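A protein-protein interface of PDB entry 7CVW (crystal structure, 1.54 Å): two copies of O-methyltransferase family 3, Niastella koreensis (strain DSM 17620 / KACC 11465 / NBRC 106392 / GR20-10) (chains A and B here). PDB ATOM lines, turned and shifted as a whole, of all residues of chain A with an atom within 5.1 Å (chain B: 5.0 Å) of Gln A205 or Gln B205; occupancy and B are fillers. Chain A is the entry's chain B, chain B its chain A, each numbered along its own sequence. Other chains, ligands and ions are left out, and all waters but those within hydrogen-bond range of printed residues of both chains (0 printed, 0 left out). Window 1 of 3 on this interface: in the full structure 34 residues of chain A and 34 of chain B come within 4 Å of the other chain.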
ATOM      1  N   PHE A   6      -7.699  25.052   2.859  1.00  0.00           N
ATOM      2  CA  PHE A   6      -8.247  25.327   1.506  1.00  0.00           C
ATOM      3  C   PHE A   6      -8.947  26.687   1.493  1.00  0.00           C
ATOM      4  O   PHE A   6      -8.888  27.407   0.469  1.00  0.00           O
ATOM      5  CB  PHE A   6      -9.208  24.233   1.044  1.00  0.00           C
ATOM      6  CG  PHE A   6      -8.613  22.852   1.044  1.00  0.00           C
ATOM      7  CD1 PHE A   6      -7.432  22.577   0.380  1.00  0.00           C
ATOM      8  CD2 PHE A   6      -9.250  21.810   1.686  1.00  0.00           C
ATOM      9  CE1 PHE A   6      -6.888  21.304   0.374  1.00  0.00           C
ATOM     10  CE2 PHE A   6      -8.701  20.539   1.690  1.00  0.00           C
ATOM     11  CZ  PHE A   6      -7.519  20.287   1.038  1.00  0.00           C
ATOM     12  N   VAL A   9      -6.150  29.393   1.625  1.00  0.00           N
ATOM     13  CA  VAL A   9      -5.484  29.501   0.303  1.00  0.00           C
ATOM     14  C   VAL A   9      -6.454  30.165  -0.675  1.00  0.00           C
ATOM     15  O   VAL A   9      -6.009  30.968  -1.506  1.00  0.00           O
ATOM     16  CB  VAL A   9      -4.999  28.130  -0.199  1.00  0.00           C
ATOM     17  CG1 VAL A   9      -4.580  28.215  -1.661  1.00  0.00           C
ATOM     18  CG2 VAL A   9      -3.865  27.565   0.657  1.00  0.00           C
ATOM     19  N   ASP A  10      -7.760  29.880  -0.607  1.00  0.00           N
ATOM     20  CA  ASP A  10      -8.711  30.541  -1.545  1.00  0.00           C
ATOM     21  C   ASP A  10      -8.691  32.066  -1.309  1.00  0.00           C
ATOM     22  O   ASP A  10      -8.701  32.827  -2.277  1.00  0.00           O
ATOM     23  CB  ASP A  10     -10.141  30.014  -1.407  1.00  0.00           C
ATOM     24  CG  ASP A  10     -10.795  29.588  -2.721  1.00  0.00           C
ATOM     25  OD1 ASP A  10     -10.060  29.363  -3.695  1.00  0.00           O
ATOM     26  OD2 ASP A  10     -12.021  29.403  -2.730  1.00  0.00           O
ATOM     27  N   ILE A  13      -5.663  33.525  -2.831  1.00  0.00           N
ATOM     28  CA  ILE A  13      -5.837  33.628  -4.313  1.00  0.00           C
ATOM     29  C   ILE A  13      -6.782  34.783  -4.669  1.00  0.00           C
ATOM     30  O   ILE A  13      -6.508  35.491  -5.634  1.00  0.00           O
ATOM     31  CB  ILE A  13      -6.327  32.299  -4.912  1.00  0.00           C
ATOM     32  CG1 ILE A  13      -5.282  31.194  -4.752  1.00  0.00           C
ATOM     33  CG2 ILE A  13      -6.696  32.481  -6.371  1.00  0.00           C
ATOM     34  CD1 ILE A  13      -5.773  29.823  -5.069  1.00  0.00           C
ATOM     35  N   ILE A 168     -18.718  16.014  -7.851  1.00  0.00           N
ATOM     36  CA  ILE A 168     -17.885  15.197  -6.909  1.00  0.00           C
ATOM     37  C   ILE A 168     -18.531  15.110  -5.518  1.00  0.00           C
ATOM     38  O   ILE A 168     -18.423  14.055  -4.852  1.00  0.00           O
ATOM     39  CB  ILE A 168     -16.441  15.759  -6.884  1.00  0.00           C
ATOM     40  CG1 ILE A 168     -15.761  15.519  -8.238  1.00  0.00           C
ATOM     41  CG2 ILE A 168     -15.636  15.193  -5.724  1.00  0.00           C
ATOM     42  CD1 ILE A 168     -15.665  14.057  -8.641  1.00  0.00           C
ATOM     43  N   ILE A 203     -12.838  15.756 -15.311  1.00  0.00           N
ATOM     44  CA  ILE A 203     -13.442  16.312 -14.087  1.00  0.00           C
ATOM     45  C   ILE A 203     -12.288  16.956 -13.320  1.00  0.00           C
ATOM     46  O   ILE A 203     -11.255  16.295 -13.069  1.00  0.00           O
ATOM     47  CB  ILE A 203     -14.246  15.272 -13.287  1.00  0.00           C
ATOM     48  CG1 ILE A 203     -15.429  14.748 -14.108  1.00  0.00           C
ATOM     49  CG2 ILE A 203     -14.691  15.876 -11.963  1.00  0.00           C
ATOM     50  CD1 ILE A 203     -16.072  13.492 -13.566  1.00  0.00           C
ATOM     51  N   LEU A 204     -12.477  18.215 -12.946  1.00  0.00           N
ATOM     52  CA  LEU A 204     -11.545  18.955 -12.058  1.00  0.00           C
ATOM     53  C   LEU A 204     -12.051  18.883 -10.630  1.00  0.00           C
ATOM     54  O   LEU A 204     -13.131  19.430 -10.348  1.00  0.00           O
ATOM     55  CB  LEU A 204     -11.463  20.429 -12.464  1.00  0.00           C
ATOM     56  CG  LEU A 204     -10.770  20.741 -13.776  1.00  0.00           C
ATOM     57  CD1 LEU A 204     -11.000  22.213 -14.102  1.00  0.00           C
ATOM     58  CD2 LEU A 204      -9.283  20.428 -13.668  1.00  0.00           C
ATOM     59  N   GLN A 205     -11.284  18.272  -9.744  1.00  0.00           N
ATOM     60  CA  GLN A 205     -11.570  18.367  -8.300  1.00  0.00           C
ATOM     61  C   GLN A 205     -11.314  19.807  -7.858  1.00  0.00           C
ATOM     62  O   GLN A 205     -10.363  20.457  -8.361  1.00  0.00           O
ATOM     63  CB  GLN A 205     -10.716  17.405  -7.477  1.00  0.00           C
ATOM     64  CG  GLN A 205     -10.843  15.941  -7.901  1.00  0.00           C
ATOM     65  CD  GLN A 205     -10.121  15.015  -6.951  1.00  0.00           C
ATOM     66  OE1 GLN A 205      -9.267  14.198  -7.337  1.00  0.00           O
ATOM     67  NE2 GLN A 205     -10.515  15.070  -5.703  1.00  0.00           N
ATOM     68  N   MET A 206     -12.172  20.291  -6.976  1.00  0.00           N
ATOM     69  CA  MET A 206     -12.153  21.706  -6.560  1.00  0.00           C
ATOM     70  C   MET A 206     -12.256  21.794  -5.049  1.00  0.00           C
ATOM     71  O   MET A 206     -13.070  21.109  -4.439  1.00  0.00           O
ATOM     72  CB  MET A 206     -13.291  22.483  -7.214  1.00  0.00           C
ATOM     73  CG  MET A 206     -13.149  22.531  -8.722  1.00  0.00           C
ATOM     74  SD  MET A 206     -14.023  23.924  -9.417  1.00  0.00           S
ATOM     75  CE  MET A 206     -13.389  23.799 -11.094  1.00  0.00           C
ATOM     76  N   VAL A 207     -11.371  22.587  -4.471  1.00  0.00           N
ATOM     77  CA  VAL A 207     -11.390  22.880  -3.025  1.00  0.00           C
ATOM     78  C   VAL A 207     -11.288  24.388  -2.873  1.00  0.00           C
ATOM     79  O   VAL A 207     -10.915  25.067  -3.851  1.00  0.00           O
ATOM     80  CB  VAL A 207     -10.247  22.152  -2.304  1.00  0.00           C
ATOM     81  CG1 VAL A 207     -10.453  20.644  -2.294  1.00  0.00           C
ATOM     82  CG2 VAL A 207      -8.885  22.499  -2.873  1.00  0.00           C
ATOM     83  N   GLY A 208     -11.588  24.873  -1.674  1.00  0.00           N
ATOM     84  CA  GLY A 208     -11.546  26.315  -1.396  1.00  0.00           C
ATOM     85  C   GLY A 208     -12.531  26.698  -0.317  1.00  0.00           C
ATOM     86  O   GLY A 208     -12.708  25.931   0.626  1.00  0.00           O
ATOM     87  N   TYR A 212     -15.668  20.660  -0.563  1.00  0.00           N
ATOM     88  CA  TYR A 212     -14.924  19.872  -1.574  1.00  0.00           C
ATOM     89  C   TYR A 212     -15.907  19.379  -2.639  1.00  0.00           C
ATOM     90  O   TYR A 212     -16.960  18.807  -2.294  1.00  0.00           O
ATOM     91  CB  TYR A 212     -14.223  18.722  -0.860  1.00  0.00           C
ATOM     92  CG  TYR A 212     -13.700  17.601  -1.705  1.00  0.00           C
ATOM     93  CD1 TYR A 212     -12.980  17.822  -2.867  1.00  0.00           C
ATOM     94  CD2 TYR A 212     -13.855  16.297  -1.270  1.00  0.00           C
ATOM     95  CE1 TYR A 212     -12.469  16.768  -3.615  1.00  0.00           C
ATOM     96  CE2 TYR A 212     -13.343  15.236  -1.997  1.00  0.00           C
ATOM     97  CZ  TYR A 212     -12.651  15.465  -3.168  1.00  0.00           C
ATOM     98  OH  TYR A 212     -12.151  14.400  -3.863  1.00  0.00           O
ATOM     99  N   ASP A 213     -15.604  19.628  -3.908  1.00  0.00           N
ATOM    100  CA  ASP A 213     -16.518  19.260  -5.007  1.00  0.00           C
ATOM    101  C   ASP A 213     -15.716  19.161  -6.308  1.00  0.00           C
ATOM    102  O   ASP A 213     -14.510  18.835  -6.257  1.00  0.00           O
ATOM    103  CB  ASP A 213     -17.664  20.271  -5.038  1.00  0.00           C
ATOM    104  CG  ASP A 213     -18.969  19.747  -5.604  1.00  0.00           C
ATOM    105  OD1 ASP A 213     -18.937  18.699  -6.300  1.00  0.00           O
ATOM    106  OD2 ASP A 213     -20.017  20.401  -5.339  1.00  0.00           O
ATOM    107  N   GLY A 214     -16.353  19.380  -7.454  1.00  0.00           N
ATOM    108  CA  GLY A 214     -15.659  19.277  -8.745  1.00  0.00           C
ATOM    109  C   GLY A 214     -16.545  19.777  -9.858  1.00  0.00           C
ATOM    110  O   GLY A 214     -17.773  19.863  -9.647  1.00  0.00           O
ATOM    111  N   PHE B   6      -8.834  12.247  -1.838  1.00  0.00           N
ATOM    112  CA  PHE B   6      -8.461  12.929  -3.107  1.00  0.00           C
ATOM    113  C   PHE B   6      -7.839  11.930  -4.087  1.00  0.00           C
ATOM    114  O   PHE B   6      -8.113  11.996  -5.298  1.00  0.00           O
ATOM    115  CB  PHE B   6      -7.538  14.120  -2.871  1.00  0.00           C
ATOM    116  CG  PHE B   6      -8.098  15.088  -1.867  1.00  0.00           C
ATOM    117  CD1 PHE B   6      -9.336  15.682  -2.054  1.00  0.00           C
ATOM    118  CD2 PHE B   6      -7.376  15.398  -0.728  1.00  0.00           C
ATOM    119  CE1 PHE B   6      -9.840  16.568  -1.117  1.00  0.00           C
ATOM    120  CE2 PHE B   6      -7.899  16.260   0.225  1.00  0.00           C
ATOM    121  CZ  PHE B   6      -9.112  16.869   0.008  1.00  0.00           C
ATOM    122  N   VAL B   9     -10.717   9.627  -5.385  1.00  0.00           N
ATOM    123  CA  VAL B   9     -11.538  10.370  -6.376  1.00  0.00           C
ATOM    124  C   VAL B   9     -10.749  10.543  -7.681  1.00  0.00           C
ATOM    125  O   VAL B   9     -11.347  10.431  -8.763  1.00  0.00           O
ATOM    126  CB  VAL B   9     -12.063  11.703  -5.816  1.00  0.00           C
ATOM    127  CG1 VAL B   9     -12.624  12.587  -6.911  1.00  0.00           C
ATOM    128  CG2 VAL B   9     -13.126  11.434  -4.761  1.00  0.00           C
ATOM    129  N   ASP B  10      -9.443  10.805  -7.594  1.00  0.00           N
ATOM    130  CA  ASP B  10      -8.625  10.957  -8.825  1.00  0.00           C
ATOM    131  C   ASP B  10      -8.691   9.644  -9.625  1.00  0.00           C
ATOM    132  O   ASP B  10      -8.837   9.705 -10.837  1.00  0.00           O
ATOM    133  CB  ASP B  10      -7.187  11.388  -8.529  1.00  0.00           C
ATOM    134  CG  ASP B  10      -6.658  12.528  -9.413  1.00  0.00           C
ATOM    135  OD1 ASP B  10      -7.464  13.271 -10.001  1.00  0.00           O
ATOM    136  OD2 ASP B  10      -5.441  12.700  -9.449  1.00  0.00           O
ATOM    137  N   ILE B  13     -12.026   9.348 -11.422  1.00  0.00           N
ATOM    138  CA  ILE B  13     -12.033  10.255 -12.600  1.00  0.00           C
ATOM    139  C   ILE B  13     -11.175   9.682 -13.729  1.00  0.00           C
ATOM    140  O   ILE B  13     -11.615   9.736 -14.865  1.00  0.00           O
ATOM    141  CB  ILE B  13     -11.574  11.678 -12.219  1.00  0.00           C
ATOM    142  CG1 ILE B  13     -12.558  12.331 -11.250  1.00  0.00           C
ATOM    143  CG2 ILE B  13     -11.378  12.508 -13.473  1.00  0.00           C
ATOM    144  CD1 ILE B  13     -12.004  13.577 -10.597  1.00  0.00           C
ATOM    145  N   ILE B 168       1.081  26.480  -5.434  1.00  0.00           N
ATOM    146  CA  ILE B 168       0.416  26.447  -4.093  1.00  0.00           C
ATOM    147  C   ILE B 168       1.236  25.636  -3.079  1.00  0.00           C
ATOM    148  O   ILE B 168       1.287  26.039  -1.909  1.00  0.00           O
ATOM    149  CB  ILE B 168      -1.042  25.953  -4.216  1.00  0.00           C
ATOM    150  CG1 ILE B 168      -1.909  26.969  -4.967  1.00  0.00           C
ATOM    151  CG2 ILE B 168      -1.641  25.632  -2.858  1.00  0.00           C
ATOM    152  CD1 ILE B 168      -1.916  28.372  -4.388  1.00  0.00           C
ATOM    153  N   ILE B 203      -5.726  31.321 -10.086  1.00  0.00           N
ATOM    154  CA  ILE B 203      -4.987  30.112  -9.655  1.00  0.00           C
ATOM    155  C   ILE B 203      -6.037  29.058  -9.305  1.00  0.00           C
ATOM    156  O   ILE B 203      -7.022  29.369  -8.560  1.00  0.00           O
ATOM    157  CB  ILE B 203      -4.033  30.398  -8.481  1.00  0.00           C
ATOM    158  CG1 ILE B 203      -2.920  31.360  -8.908  1.00  0.00           C
ATOM    159  CG2 ILE B 203      -3.489  29.100  -7.920  1.00  0.00           C
ATOM    160  CD1 ILE B 203      -2.232  32.053  -7.743  1.00  0.00           C
ATOM    161  N   LEU B 204      -5.891  27.868  -9.865  1.00  0.00           N
ATOM    162  CA  LEU B 204      -6.779  26.722  -9.569  1.00  0.00           C
ATOM    163  C   LEU B 204      -6.097  25.860  -8.530  1.00  0.00           C
ATOM    164  O   LEU B 204      -5.054  25.275  -8.854  1.00  0.00           O
ATOM    165  CB  LEU B 204      -6.978  25.831 -10.795  1.00  0.00           C
ATOM    166  CG  LEU B 204      -7.904  26.333 -11.875  1.00  0.00           C
ATOM    167  CD1 LEU B 204      -7.818  25.413 -13.101  1.00  0.00           C
ATOM    168  CD2 LEU B 204      -9.330  26.387 -11.351  1.00  0.00           C
ATOM    169  N   GLN B 205      -6.712  25.707  -7.372  1.00  0.00           N
ATOM    170  CA  GLN B 205      -6.265  24.727  -6.374  1.00  0.00           C
ATOM    171  C   GLN B 205      -6.461  23.327  -6.954  1.00  0.00           C
ATOM    172  O   GLN B 205      -7.505  23.070  -7.592  1.00  0.00           O
ATOM    173  CB  GLN B 205      -7.005  24.906  -5.061  1.00  0.00           C
ATOM    174  CG  GLN B 205      -6.805  26.273  -4.425  1.00  0.00           C
ATOM    175  CD  GLN B 205      -7.302  26.339  -3.001  1.00  0.00           C
ATOM    176  OE1 GLN B 205      -8.117  27.204  -2.628  1.00  0.00           O
ATOM    177  NE2 GLN B 205      -6.782  25.454  -2.184  1.00  0.00           N
ATOM    178  N   MET B 206      -5.492  22.454  -6.727  1.00  0.00           N
ATOM    179  CA  MET B 206      -5.572  21.078  -7.261  1.00  0.00           C
ATOM    180  C   MET B 206      -5.266  20.047  -6.188  1.00  0.00           C
ATOM    181  O   MET B 206      -4.325  20.205  -5.406  1.00  0.00           O
ATOM    182  CB  MET B 206      -4.646  20.910  -8.455  1.00  0.00           C
ATOM    183  CG  MET B 206      -5.163  21.700  -9.641  1.00  0.00           C
ATOM    184  SD  MET B 206      -4.263  21.266 -11.128  1.00  0.00           S
ATOM    185  CE  MET B 206      -5.109  22.345 -12.286  1.00  0.00           C
ATOM    186  N   VAL B 207      -6.094  19.003  -6.197  1.00  0.00           N
ATOM    187  CA  VAL B 207      -5.923  17.813  -5.328  1.00  0.00           C
ATOM    188  C   VAL B 207      -6.067  16.567  -6.197  1.00  0.00           C
ATOM    189  O   VAL B 207      -6.577  16.653  -7.334  1.00  0.00           O
ATOM    190  CB  VAL B 207      -6.908  17.824  -4.147  1.00  0.00           C
ATOM    191  CG1 VAL B 207      -6.605  18.987  -3.219  1.00  0.00           C
ATOM    192  CG2 VAL B 207      -8.358  17.877  -4.610  1.00  0.00           C
ATOM    193  N   GLY B 208      -5.572  15.444  -5.698  1.00  0.00           N
ATOM    194  CA  GLY B 208      -5.621  14.173  -6.430  1.00  0.00           C
ATOM    195  C   GLY B 208      -4.506  13.261  -5.989  1.00  0.00           C
ATOM    196  O   GLY B 208      -4.200  13.226  -4.812  1.00  0.00           O
ATOM    197  N   TYR B 212      -1.373  18.167  -2.667  1.00  0.00           N
ATOM    198  CA  TYR B 212      -2.159  19.406  -2.785  1.00  0.00           C
ATOM    199  C   TYR B 212      -1.269  20.514  -3.366  1.00  0.00           C
ATOM    200  O   TYR B 212      -0.165  20.790  -2.833  1.00  0.00           O
ATOM    201  CB  TYR B 212      -2.693  19.765  -1.399  1.00  0.00           C
ATOM    202  CG  TYR B 212      -3.283  21.146  -1.237  1.00  0.00           C
ATOM    203  CD1 TYR B 212      -4.166  21.703  -2.146  1.00  0.00           C
ATOM    204  CD2 TYR B 212      -2.992  21.876  -0.095  1.00  0.00           C
ATOM    205  CE1 TYR B 212      -4.716  22.960  -1.945  1.00  0.00           C
ATOM    206  CE2 TYR B 212      -3.581  23.101   0.141  1.00  0.00           C
ATOM    207  CZ  TYR B 212      -4.412  23.667  -0.796  1.00  0.00           C
ATOM    208  OH  TYR B 212      -4.973  24.885  -0.566  1.00  0.00           O
ATOM    209  N   ASP B 213      -1.756  21.155  -4.417  1.00  0.00           N
ATOM    210  CA  ASP B 213      -0.968  22.175  -5.135  1.00  0.00           C
ATOM    211  C   ASP B 213      -1.935  23.021  -5.956  1.00  0.00           C
ATOM    212  O   ASP B 213      -3.071  23.229  -5.558  1.00  0.00           O
ATOM    213  CB  ASP B 213       0.124  21.470  -5.950  1.00  0.00           C
ATOM    214  CG  ASP B 213       1.371  22.276  -6.249  1.00  0.00           C
ATOM    215  OD1 ASP B 213       1.336  23.491  -6.110  1.00  0.00           O
ATOM    216  OD2 ASP B 213       2.383  21.658  -6.593  1.00  0.00           O
ATOM    217  N   GLY B 214      -1.464  23.582  -7.050  1.00  0.00           N
ATOM    218  CA  GLY B 214      -2.320  24.409  -7.900  1.00  0.00           C
ATOM    219  C   GLY B 214      -1.588  24.836  -9.148  1.00  0.00           C
ATOM    220  O   GLY B 214      -0.340  24.781  -9.208  1.00  0.00           O
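The side-chain carboxylate (OD1) of Asp A10 sits close to the side-chain amide oxygen (OE1) of Gln B205 (3.1 Å). The side-chain amide oxygen (OE1) of Gln A205 lies close to the side-chain carboxylate (OD1) of Asp B10 (3.3 Å). The side-chain amide oxygen of Gln A205 sits close to the backbone carbonyl oxygen of Phe B6 (3.2 Å). The backbone carbonyl oxygen (O) of Phe A6 lies close to the side-chain amide oxygen (OE1) of Gln B205, at 3.2 Å.
The side-chain carboxylate (OD1) of Asp A213 is in hydrogen-bond range of the backbone NH (N) of Ile A168 (3.1 Å). NE2 of Gln B205 lies within hydrogen-bond range of OH of Tyr B212 (2.5 Å). OH of Tyr A212 is in hydrogen-bond range of NE2 of Gln A205, 2.6 Å away. N of Ile B168 is in hydrogen-bond range of OD1 of Asp B213 (3.1 Å).
Phe A6 touches Phe B6. Ile B168 touches Val A9 (CD1 to CG1, 3.8 Å). Gln B205 touches Val A9. CD1 of Ile A13 touches CG of Gln B205, 3.8 Å away. Val B9 touches Ile A168 (CG1 to CD1, 3.8 Å). Ile A203 touches Ile B13. Gln A205 touches Val B9. Gln A205 touches Gln B205 (O to O, 3.9 Å). Tyr A212 touches Phe B6. OH of Tyr A212 touches CG2 of Val B9, 3.2 Å away.
Leu A204 touches none of the printed residues of chain B. Gln A205 touches just these residues of chain B: Phe B6 (3.2 Å), Val B9 (3.5 Å), Asp B10 (3.3 Å), Ile B13 (3.8 Å), Gln B205 (3.9 Å), Val B207 (3.6 Å) and Gly B208 (3.8 Å). Met A206 touches none of the printed residues of chain B. Of the printed residues of chain B, Tyr A212 touches Phe B6 and Val B9. Of the printed residues of chain A, Phe B6 touches Phe A6, Gln A205 and Tyr A212. Of the printed residues of chain A, Gln B205 touches Phe A6 (3.2 Å), Val A9 (3.6 Å), Asp A10 (3.1 Å), Ile A13 (3.8 Å), Gln A205 (3.9 Å), Val A207 (3.7 Å) and Gly A208 (3.8 Å). Of the printed residues of chain A, Gly B208 touches Gln A205. The nearest printed residue of chain B that does not touch Phe A6 is Val B207 (4.3 Å).
Hydrophobic or aromatic side chains of chain B within 4 Å of the printed part of chain A: Phe B6, Val B9, Ile B13, Ile B168, Ile B203, Val B207 and Tyr B212. Hydrophobic or aromatic side chains of chain A within 4 Å of the printed part of chain B: Phe A6, Val A9, Ile A13, Ile A168, Ile A203, Val A207 and Tyr A212. Among the printed residues, no Asp or Glu carboxylate lies within 4 Å of a Lys or Arg side-chain nitrogen of the other chain.
Phe A6 touches Gln B205, and with the chains exchanged Gln A205 touches Phe B6. Phe A6 touches Tyr B212, and with the chains exchanged Tyr A212 touches Phe B6. Gln A205 touches its own counterpart, Gln B205. Gln A205 touches Val B207, and with the chains exchanged Val A207 touches Gln B205.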
